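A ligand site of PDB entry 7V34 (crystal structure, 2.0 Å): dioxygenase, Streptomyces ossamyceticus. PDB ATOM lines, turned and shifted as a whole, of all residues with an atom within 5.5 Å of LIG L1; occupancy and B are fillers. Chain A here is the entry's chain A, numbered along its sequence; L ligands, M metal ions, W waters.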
ATOM      1  N   LEU A 108      -3.417 -23.872  -7.513  1.00  0.00           N
ATOM      2  CA  LEU A 108      -3.966 -22.603  -7.053  1.00  0.00           C
ATOM      3  C   LEU A 108      -2.917 -21.501  -6.952  1.00  0.00           C
ATOM      4  O   LEU A 108      -3.294 -20.325  -6.872  1.00  0.00           O
ATOM      5  CB  LEU A 108      -4.632 -22.791  -5.684  1.00  0.00           C
ATOM      6  CG  LEU A 108      -5.741 -23.855  -5.622  1.00  0.00           C
ATOM      7  CD1 LEU A 108      -6.225 -24.039  -4.186  1.00  0.00           C
ATOM      8  CD2 LEU A 108      -6.892 -23.475  -6.535  1.00  0.00           C
ATOM      9  N   LEU A 109      -1.634 -21.846  -6.938  1.00  0.00           N
ATOM     10  CA  LEU A 109      -0.588 -20.920  -6.528  1.00  0.00           C
ATOM     11  C   LEU A 109       0.195 -20.383  -7.738  1.00  0.00           C
ATOM     12  O   LEU A 109       0.052 -20.869  -8.853  1.00  0.00           O
ATOM     13  CB  LEU A 109       0.374 -21.617  -5.563  1.00  0.00           C
ATOM     14  CG  LEU A 109      -0.270 -22.190  -4.290  1.00  0.00           C
ATOM     15  CD1 LEU A 109       0.816 -22.689  -3.357  1.00  0.00           C
ATOM     16  CD2 LEU A 109      -1.121 -21.131  -3.591  1.00  0.00           C
ATOM     17  N   ARG A 114      -6.339 -14.060 -15.126  1.00  0.00           N
ATOM     18  CA  ARG A 114      -7.749 -14.403 -15.066  1.00  0.00           C
ATOM     19  C   ARG A 114      -8.471 -13.953 -16.343  1.00  0.00           C
ATOM     20  O   ARG A 114      -7.947 -13.187 -17.152  1.00  0.00           O
ATOM     21  CB  ARG A 114      -8.416 -13.773 -13.836  1.00  0.00           C
ATOM     22  CG  ARG A 114      -7.750 -14.124 -12.505  1.00  0.00           C
ATOM     23  CD  ARG A 114      -7.686 -15.631 -12.292  1.00  0.00           C
ATOM     24  NE  ARG A 114      -7.268 -15.951 -10.928  1.00  0.00           N
ATOM     25  CZ  ARG A 114      -6.947 -17.163 -10.483  1.00  0.00           C
ATOM     26  NH1 ARG A 114      -6.973 -18.215 -11.305  1.00  0.00           N
ATOM     27  NH2 ARG A 114      -6.601 -17.323  -9.216  1.00  0.00           N
ATOM     28  N   LEU A 118      -8.283  -8.761 -14.063  1.00  0.00           N
ATOM     29  CA  LEU A 118      -7.343  -9.162 -13.012  1.00  0.00           C
ATOM     30  C   LEU A 118      -6.308 -10.177 -13.482  1.00  0.00           C
ATOM     31  O   LEU A 118      -6.620 -11.162 -14.150  1.00  0.00           O
ATOM     32  CB  LEU A 118      -8.147  -9.764 -11.869  1.00  0.00           C
ATOM     33  CG  LEU A 118      -7.419 -10.319 -10.650  1.00  0.00           C
ATOM     34  CD1 LEU A 118      -6.732  -9.169  -9.936  1.00  0.00           C
ATOM     35  CD2 LEU A 118      -8.443 -10.969  -9.760  1.00  0.00           C
ATOM     36  N   GLN A 120      -3.120 -12.223 -11.097  1.00  0.00           N
ATOM     37  CA  GLN A 120      -2.797 -12.409  -9.678  1.00  0.00           C
ATOM     38  C   GLN A 120      -1.487 -13.155  -9.479  1.00  0.00           C
ATOM     39  O   GLN A 120      -1.056 -13.934 -10.335  1.00  0.00           O
ATOM     40  CB  GLN A 120      -3.891 -13.221  -8.952  1.00  0.00           C
ATOM     41  CG  GLN A 120      -5.186 -12.507  -8.857  1.00  0.00           C
ATOM     42  CD  GLN A 120      -6.184 -13.283  -8.042  1.00  0.00           C
ATOM     43  OE1 GLN A 120      -6.598 -14.369  -8.443  1.00  0.00           O
ATOM     44  NE2 GLN A 120      -6.561 -12.747  -6.876  1.00  0.00           N
ATOM     45  N   LEU A 122      -0.538 -15.664  -6.270  1.00  0.00           N
ATOM     46  CA  LEU A 122      -1.101 -16.246  -5.058  1.00  0.00           C
ATOM     47  C   LEU A 122      -0.056 -17.159  -4.436  1.00  0.00           C
ATOM     48  O   LEU A 122       0.536 -17.988  -5.138  1.00  0.00           O
ATOM     49  CB  LEU A 122      -2.383 -17.053  -5.348  1.00  0.00           C
ATOM     50  CG  LEU A 122      -3.508 -16.384  -6.152  1.00  0.00           C
ATOM     51  CD1 LEU A 122      -3.381 -16.663  -7.662  1.00  0.00           C
ATOM     52  CD2 LEU A 122      -4.888 -16.819  -5.647  1.00  0.00           C
ATOM     53  N   HIS A 180      -3.276 -17.357   2.344  1.00  0.00           N
ATOM     54  CA  HIS A 180      -2.741 -16.910   1.067  1.00  0.00           C
ATOM     55  C   HIS A 180      -2.517 -15.408   1.127  1.00  0.00           C
ATOM     56  O   HIS A 180      -3.429 -14.649   1.454  1.00  0.00           O
ATOM     57  CB  HIS A 180      -3.672 -17.272  -0.083  1.00  0.00           C
ATOM     58  CG  HIS A 180      -3.769 -18.741  -0.333  1.00  0.00           C
ATOM     59  ND1 HIS A 180      -4.613 -19.572   0.379  1.00  0.00           N
ATOM     60  CD2 HIS A 180      -3.122 -19.551  -1.221  1.00  0.00           C
ATOM     61  CE1 HIS A 180      -4.489 -20.813  -0.055  1.00  0.00           C
ATOM     62  NE2 HIS A 180      -3.590 -20.825  -1.021  1.00  0.00           N
ATOM     63  N   THR A 182      -1.958 -12.658  -1.470  1.00  0.00           N
ATOM     64  CA  THR A 182      -2.304 -12.668  -2.882  1.00  0.00           C
ATOM     65  C   THR A 182      -2.268 -11.242  -3.411  1.00  0.00           C
ATOM     66  O   THR A 182      -2.878 -10.350  -2.814  1.00  0.00           O
ATOM     67  CB  THR A 182      -3.694 -13.268  -3.091  1.00  0.00           C
ATOM     68  OG1 THR A 182      -3.642 -14.661  -2.766  1.00  0.00           O
ATOM     69  CG2 THR A 182      -4.198 -13.087  -4.541  1.00  0.00           C
ATOM     70  N   ASN A 184      -2.790  -8.487  -6.600  1.00  0.00           N
ATOM     71  CA  ASN A 184      -3.745  -8.271  -7.683  1.00  0.00           C
ATOM     72  C   ASN A 184      -3.321  -7.080  -8.536  1.00  0.00           C
ATOM     73  O   ASN A 184      -2.967  -6.032  -8.000  1.00  0.00           O
ATOM     74  CB  ASN A 184      -5.147  -7.965  -7.133  1.00  0.00           C
ATOM     75  CG  ASN A 184      -5.726  -9.104  -6.334  1.00  0.00           C
ATOM     76  OD1 ASN A 184      -5.445 -10.269  -6.580  1.00  0.00           O
ATOM     77  ND2 ASN A 184      -6.556  -8.764  -5.374  1.00  0.00           N
ATOM     78  N   LEU A 195     -13.025  -7.436 -11.735  1.00  0.00           N
ATOM     79  CA  LEU A 195     -13.098  -8.766 -11.141  1.00  0.00           C
ATOM     80  C   LEU A 195     -14.576  -9.062 -10.940  1.00  0.00           C
ATOM     81  O   LEU A 195     -15.284  -8.248 -10.347  1.00  0.00           O
ATOM     82  CB  LEU A 195     -12.320  -8.853  -9.811  1.00  0.00           C
ATOM     83  CG  LEU A 195     -12.567 -10.055  -8.896  1.00  0.00           C
ATOM     84  CD1 LEU A 195     -12.279 -11.385  -9.605  1.00  0.00           C
ATOM     85  CD2 LEU A 195     -11.722  -9.948  -7.618  1.00  0.00           C
ATOM     86  N   HIS A 198     -18.412 -11.862  -6.708  1.00  0.00           N
ATOM     87  CA  HIS A 198     -18.050 -13.115  -6.065  1.00  0.00           C
ATOM     88  C   HIS A 198     -18.081 -12.945  -4.550  1.00  0.00           C
ATOM     89  O   HIS A 198     -18.100 -11.834  -4.012  1.00  0.00           O
ATOM     90  CB  HIS A 198     -16.656 -13.584  -6.497  1.00  0.00           C
ATOM     91  CG  HIS A 198     -15.565 -12.727  -5.955  1.00  0.00           C
ATOM     92  ND1 HIS A 198     -15.310 -11.457  -6.431  1.00  0.00           N
ATOM     93  CD2 HIS A 198     -14.704 -12.926  -4.931  1.00  0.00           C
ATOM     94  CE1 HIS A 198     -14.327 -10.917  -5.745  1.00  0.00           C
ATOM     95  NE2 HIS A 198     -13.939 -11.790  -4.826  1.00  0.00           N
ATOM     96  N   LYS A 199     -18.050 -14.078  -3.873  1.00  0.00           N
ATOM     97  CA  LYS A 199     -17.743 -14.185  -2.457  1.00  0.00           C
ATOM     98  C   LYS A 199     -16.390 -14.852  -2.324  1.00  0.00           C
ATOM     99  O   LYS A 199     -16.048 -15.745  -3.110  1.00  0.00           O
ATOM    100  CB  LYS A 199     -18.821 -15.013  -1.739  1.00  0.00           C
ATOM    101  CG  LYS A 199     -20.221 -14.353  -1.763  1.00  0.00           C
ATOM    102  CD  LYS A 199     -21.308 -15.339  -1.324  1.00  0.00           C
ATOM    103  CE  LYS A 199     -22.609 -14.643  -0.951  1.00  0.00           C
ATOM    104  NZ  LYS A 199     -23.547 -15.582  -0.274  1.00  0.00           N
ATOM    105  N   ASP A 200     -15.591 -14.404  -1.349  1.00  0.00           N
ATOM    106  CA  ASP A 200     -14.329 -15.078  -1.065  1.00  0.00           C
ATOM    107  C   ASP A 200     -14.584 -16.450  -0.468  1.00  0.00           C
ATOM    108  O   ASP A 200     -15.672 -16.734   0.048  1.00  0.00           O
ATOM    109  CB  ASP A 200     -13.466 -14.237  -0.125  1.00  0.00           C
ATOM    110  CG  ASP A 200     -13.000 -12.954  -0.772  1.00  0.00           C
ATOM    111  OD1 ASP A 200     -13.098 -12.905  -2.012  1.00  0.00           O
ATOM    112  OD2 ASP A 200     -12.543 -12.015  -0.096  1.00  0.00           O
ATOM    113  N   ASP A 201     -13.573 -17.319  -0.521  1.00  0.00           N
ATOM    114  CA  ASP A 201     -13.762 -18.704  -0.086  1.00  0.00           C
ATOM    115  C   ASP A 201     -13.782 -18.885   1.431  1.00  0.00           C
ATOM    116  O   ASP A 201     -14.470 -19.782   1.924  1.00  0.00           O
ATOM    117  CB  ASP A 201     -12.654 -19.580  -0.622  1.00  0.00           C
ATOM    118  CG  ASP A 201     -11.360 -19.363   0.142  1.00  0.00           C
ATOM    119  OD1 ASP A 201     -10.820 -18.249   0.038  1.00  0.00           O
ATOM    120  OD2 ASP A 201     -10.927 -20.273   0.880  1.00  0.00           O
ATOM    121  N   PHE A 271      -5.717 -13.857   2.940  1.00  0.00           N
ATOM    122  CA  PHE A 271      -6.889 -14.710   2.951  1.00  0.00           C
ATOM    123  C   PHE A 271      -6.660 -15.857   3.933  1.00  0.00           C
ATOM    124  O   PHE A 271      -5.616 -16.519   3.870  1.00  0.00           O
ATOM    125  CB  PHE A 271      -7.171 -15.291   1.557  1.00  0.00           C
ATOM    126  CG  PHE A 271      -7.544 -14.244   0.517  1.00  0.00           C
ATOM    127  CD1 PHE A 271      -6.570 -13.445  -0.065  1.00  0.00           C
ATOM    128  CD2 PHE A 271      -8.873 -14.094   0.111  1.00  0.00           C
ATOM    129  CE1 PHE A 271      -6.918 -12.488  -1.042  1.00  0.00           C
ATOM    130  CE2 PHE A 271      -9.227 -13.161  -0.867  1.00  0.00           C
ATOM    131  CZ  PHE A 271      -8.250 -12.350  -1.430  1.00  0.00           C
ATOM    132  N   SER A 273      -8.157 -19.461   5.325  1.00  0.00           N
ATOM    133  CA  SER A 273      -9.034 -20.557   4.969  1.00  0.00           C
ATOM    134  C   SER A 273      -8.767 -21.737   5.875  1.00  0.00           C
ATOM    135  O   SER A 273      -7.672 -21.865   6.435  1.00  0.00           O
ATOM    136  CB  SER A 273      -8.843 -20.984   3.497  1.00  0.00           C
ATOM    137  OG  SER A 273      -8.942 -19.834   2.661  1.00  0.00           O
ATOM    138  N   CYS A 276      -6.096 -26.271   3.788  1.00  0.00           N
ATOM    139  CA  CYS A 276      -6.475 -26.899   2.519  1.00  0.00           C
ATOM    140  C   CYS A 276      -5.258 -27.400   1.743  1.00  0.00           C
ATOM    141  O   CYS A 276      -5.241 -27.343   0.506  1.00  0.00           O
ATOM    142  CB  CYS A 276      -7.271 -25.918   1.660  1.00  0.00           C
ATOM    143  SG  CYS A 276      -6.392 -24.346   1.297  1.00  0.00           S
ATOM    144  N   ILE A 303     -13.011 -24.095  -2.448  1.00  0.00           N
ATOM    145  CA  ILE A 303     -12.283 -23.128  -3.272  1.00  0.00           C
ATOM    146  C   ILE A 303     -12.460 -23.443  -4.758  1.00  0.00           C
ATOM    147  O   ILE A 303     -12.705 -22.533  -5.570  1.00  0.00           O
ATOM    148  CB  ILE A 303     -10.793 -23.118  -2.886  1.00  0.00           C
ATOM    149  CG1 ILE A 303     -10.619 -22.647  -1.433  1.00  0.00           C
ATOM    150  CG2 ILE A 303      -9.989 -22.242  -3.847  1.00  0.00           C
ATOM    151  CD1 ILE A 303      -9.255 -22.996  -0.835  1.00  0.00           C
ATOM    152  N   ASN A 306     -15.974 -22.661  -5.878  1.00  0.00           N
ATOM    153  CA  ASN A 306     -16.212 -21.221  -5.899  1.00  0.00           C
ATOM    154  C   ASN A 306     -15.534 -20.586  -7.110  1.00  0.00           C
ATOM    155  O   ASN A 306     -16.145 -19.803  -7.830  1.00  0.00           O
ATOM    156  CB  ASN A 306     -15.716 -20.583  -4.603  1.00  0.00           C
ATOM    157  CG  ASN A 306     -16.226 -19.168  -4.408  1.00  0.00           C
ATOM    158  OD1 ASN A 306     -17.378 -18.862  -4.691  1.00  0.00           O
ATOM    159  ND2 ASN A 306     -15.347 -18.288  -3.925  1.00  0.00           N
ATOM    160  N   ASP A 307     -14.253 -20.923  -7.334  1.00  0.00           N
ATOM    161  CA  ASP A 307     -13.533 -20.373  -8.478  1.00  0.00           C
ATOM    162  C   ASP A 307     -14.204 -20.763  -9.792  1.00  0.00           C
ATOM    163  O   ASP A 307     -14.197 -19.970 -10.744  1.00  0.00           O
ATOM    164  CB  ASP A 307     -12.073 -20.850  -8.466  1.00  0.00           C
ATOM    165  CG  ASP A 307     -11.237 -20.207  -7.346  1.00  0.00           C
ATOM    166  OD1 ASP A 307     -11.794 -19.458  -6.510  1.00  0.00           O
ATOM    167  OD2 ASP A 307     -10.010 -20.459  -7.311  1.00  0.00           O
ATOM    168  N   ILE A 310     -17.265 -18.443 -10.101  1.00  0.00           N
ATOM    169  CA  ILE A 310     -16.881 -17.038 -10.289  1.00  0.00           C
ATOM    170  C   ILE A 310     -16.463 -16.789 -11.728  1.00  0.00           C
ATOM    171  O   ILE A 310     -17.178 -16.124 -12.480  1.00  0.00           O
ATOM    172  CB  ILE A 310     -15.707 -16.640  -9.372  1.00  0.00           C
ATOM    173  CG1 ILE A 310     -16.106 -16.735  -7.893  1.00  0.00           C
ATOM    174  CG2 ILE A 310     -15.204 -15.238  -9.731  1.00  0.00           C
ATOM    175  CD1 ILE A 310     -14.917 -16.550  -6.980  1.00  0.00           C
ATOM    176  N   TYR A 311     -15.277 -17.300 -12.094  1.00  0.00           N
ATOM    177  CA  TYR A 311     -14.597 -17.057 -13.355  1.00  0.00           C
ATOM    178  C   TYR A 311     -15.259 -17.760 -14.530  1.00  0.00           C
ATOM    179  O   TYR A 311     -14.570 -17.791 -15.566  1.00  0.00           O
ATOM    180  CB  TYR A 311     -13.130 -17.449 -13.242  1.00  0.00           C
ATOM    181  CG  TYR A 311     -12.323 -16.605 -12.253  1.00  0.00           C
ATOM    182  CD1 TYR A 311     -12.366 -15.214 -12.292  1.00  0.00           C
ATOM    183  CD2 TYR A 311     -11.539 -17.208 -11.290  1.00  0.00           C
ATOM    184  CE1 TYR A 311     -11.615 -14.448 -11.388  1.00  0.00           C
ATOM    185  CE2 TYR A 311     -10.796 -16.461 -10.378  1.00  0.00           C
ATOM    186  CZ  TYR A 311     -10.842 -15.082 -10.436  1.00  0.00           C
ATOM    187  OH  TYR A 311     -10.102 -14.372  -9.527  1.00  0.00           O
HETATM  188  C1  LIG L   1      -9.961 -16.392  -5.964  1.00  0.00           C
HETATM  189  C2  LIG L   1     -10.208 -14.884  -6.004  1.00  0.00           C
HETATM  190  C3  LIG L   1      -9.584 -14.376  -4.607  1.00  0.00           C
HETATM  191  C4  LIG L   1      -8.989 -15.669  -3.935  1.00  0.00           C
HETATM  192  C5  LIG L   1      -9.816 -16.350  -2.803  1.00  0.00           C
HETATM  193  C6  LIG L   1      -6.996 -16.099  -2.448  1.00  0.00           C
HETATM  194  C7  LIG L   1      -7.305 -18.979  -3.284  1.00  0.00           C
HETATM  195  C8  LIG L   1      -6.506 -20.248  -3.611  1.00  0.00           C
HETATM  196  C9  LIG L   1     -11.700 -14.569  -6.203  1.00  0.00           C
HETATM  197  C10 LIG L   1      -7.739 -17.131  -1.554  1.00  0.00           C
HETATM  198  C11 LIG L   1      -7.186 -18.563  -1.820  1.00  0.00           C
HETATM  199  C12 LIG L   1      -7.931 -19.589  -0.918  1.00  0.00           C
HETATM  200  N1  LIG L   1      -7.631 -15.487  -3.505  1.00  0.00           N
HETATM  201  N2  LIG L   1      -9.183 -16.990  -1.755  1.00  0.00           N
HETATM  202  O1  LIG L   1      -9.478 -14.329  -7.025  1.00  0.00           O
HETATM  203  O2  LIG L   1      -8.522 -13.483  -4.793  1.00  0.00           O
HETATM  204  O3  LIG L   1      -9.003 -16.654  -4.975  1.00  0.00           O
HETATM  205  O4  LIG L   1     -11.052 -16.313  -2.826  1.00  0.00           O
HETATM  206  O5  LIG L   1      -5.834 -15.770  -2.277  1.00  0.00           O
HETATM  207  C1  LG2 L   2     -10.146 -10.661  -4.267  1.00  0.00           C
HETATM  208  O1  LG2 L   2     -10.847 -11.645  -3.935  1.00  0.00           O
HETATM  209  O2  LG2 L   2      -8.946 -10.825  -4.526  1.00  0.00           O
HETATM  210  C2  LG2 L   2     -10.720  -9.325  -4.369  1.00  0.00           C
HETATM  211  O3  LG2 L   2     -11.900  -9.128  -4.134  1.00  0.00           O
HETATM  212  C3  LG2 L   2      -9.845  -8.145  -4.760  1.00  0.00           C
HETATM  213  C4  LG2 L   2     -10.652  -6.865  -4.491  1.00  0.00           C
HETATM  214  C5  LG2 L   2      -9.825  -5.637  -4.856  1.00  0.00           C
HETATM  215  O4  LG2 L   2     -10.109  -4.549  -4.333  1.00  0.00           O
HETATM  216  O5  LG2 L   2      -8.855  -5.751  -5.649  1.00  0.00           O
HETATM  217 FE    FE M   1     -12.755 -11.002  -3.095  1.00  0.00          FE
HETATM  218  O   HOH W   1     -12.341 -18.953  -3.742  1.00  0.00           O
HETATM  219  O   HOH W   2      -8.144 -19.163  -6.422  1.00  0.00           O
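OH of Tyr 311 is in hydrogen-bond range of O1 of LIG L1 (2.6 Å). The side-chain amide nitrogen of Gln 120 sits at hydrogen-bond distance from an oxygen (O2) of LIG L1, at 3.0 Å. OD1 of Asp 201 is in hydrogen-bond range of N2 of LIG L1, at 2.7 Å. The side-chain hydroxyl of Thr 182 sits at hydrogen-bond distance from an oxygen (O5) of LIG L1 (2.5 Å). An oxygen (O2) of LG2 L2 lies within hydrogen-bond range of the side-chain amide nitrogen of Asn 184 (3.3 Å).
An oxygen (O2) of LG2 L2 sits at hydrogen-bond distance from an oxygen (O2) of LIG L1 (2.7 Å).
OE1 of Gln 120 sits at hydrogen-bond distance from NE of Arg 114 (3.0 Å). The side-chain amide nitrogen of Gln 120 sits at hydrogen-bond distance from the side-chain amide oxygen of Asn 184, 2.7 Å away. The backbone carbonyl oxygen (O) of His 180 sits at hydrogen-bond distance from the backbone NH (N) of Phe 271. OG of Ser 273 is in hydrogen-bond range of OD2 of Asp 201.
CB of Leu 108 touches C8 of LIG L1, at 3.8 Å. Leu 122 touches LIG L1. CB of His 180 touches O5 of LIG L1, at 3.4 Å. His 198 touches LIG L1 (CD2 to C9, 3.7 Å). Asp 200 touches LIG L1. Phe 271 touches LIG L1. Ser 273 touches LIG L1. Ile 303 touches LIG L1 (CD1 to C12, 3.7 Å). OD1 of Asp 307 touches C1 of LIG L1 (3.6 Å). Ile 310 touches LIG L1 (CD1 to C9, 3.9 Å). Hydrophobic or aromatic side chains within 4 Å of LIG L1: Leu 108, Leu 122, His 180, His 198, Phe 271, Ile 303, Ile 310 and Tyr 311.
Water W2 lies within hydrogen-bond range of the side-chain carboxylate (OD2) of Asp 307 (2.4 Å) and an oxygen (O3) of LIG L1 (3.0 Å). Water W1 lies within hydrogen-bond range of the side-chain carboxylate of Asp 307 (2.9 Å), an oxygen (O4) of LIG L1 (3.1 Å) and the side-chain amide nitrogen of Asn 306 (3.1 Å).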
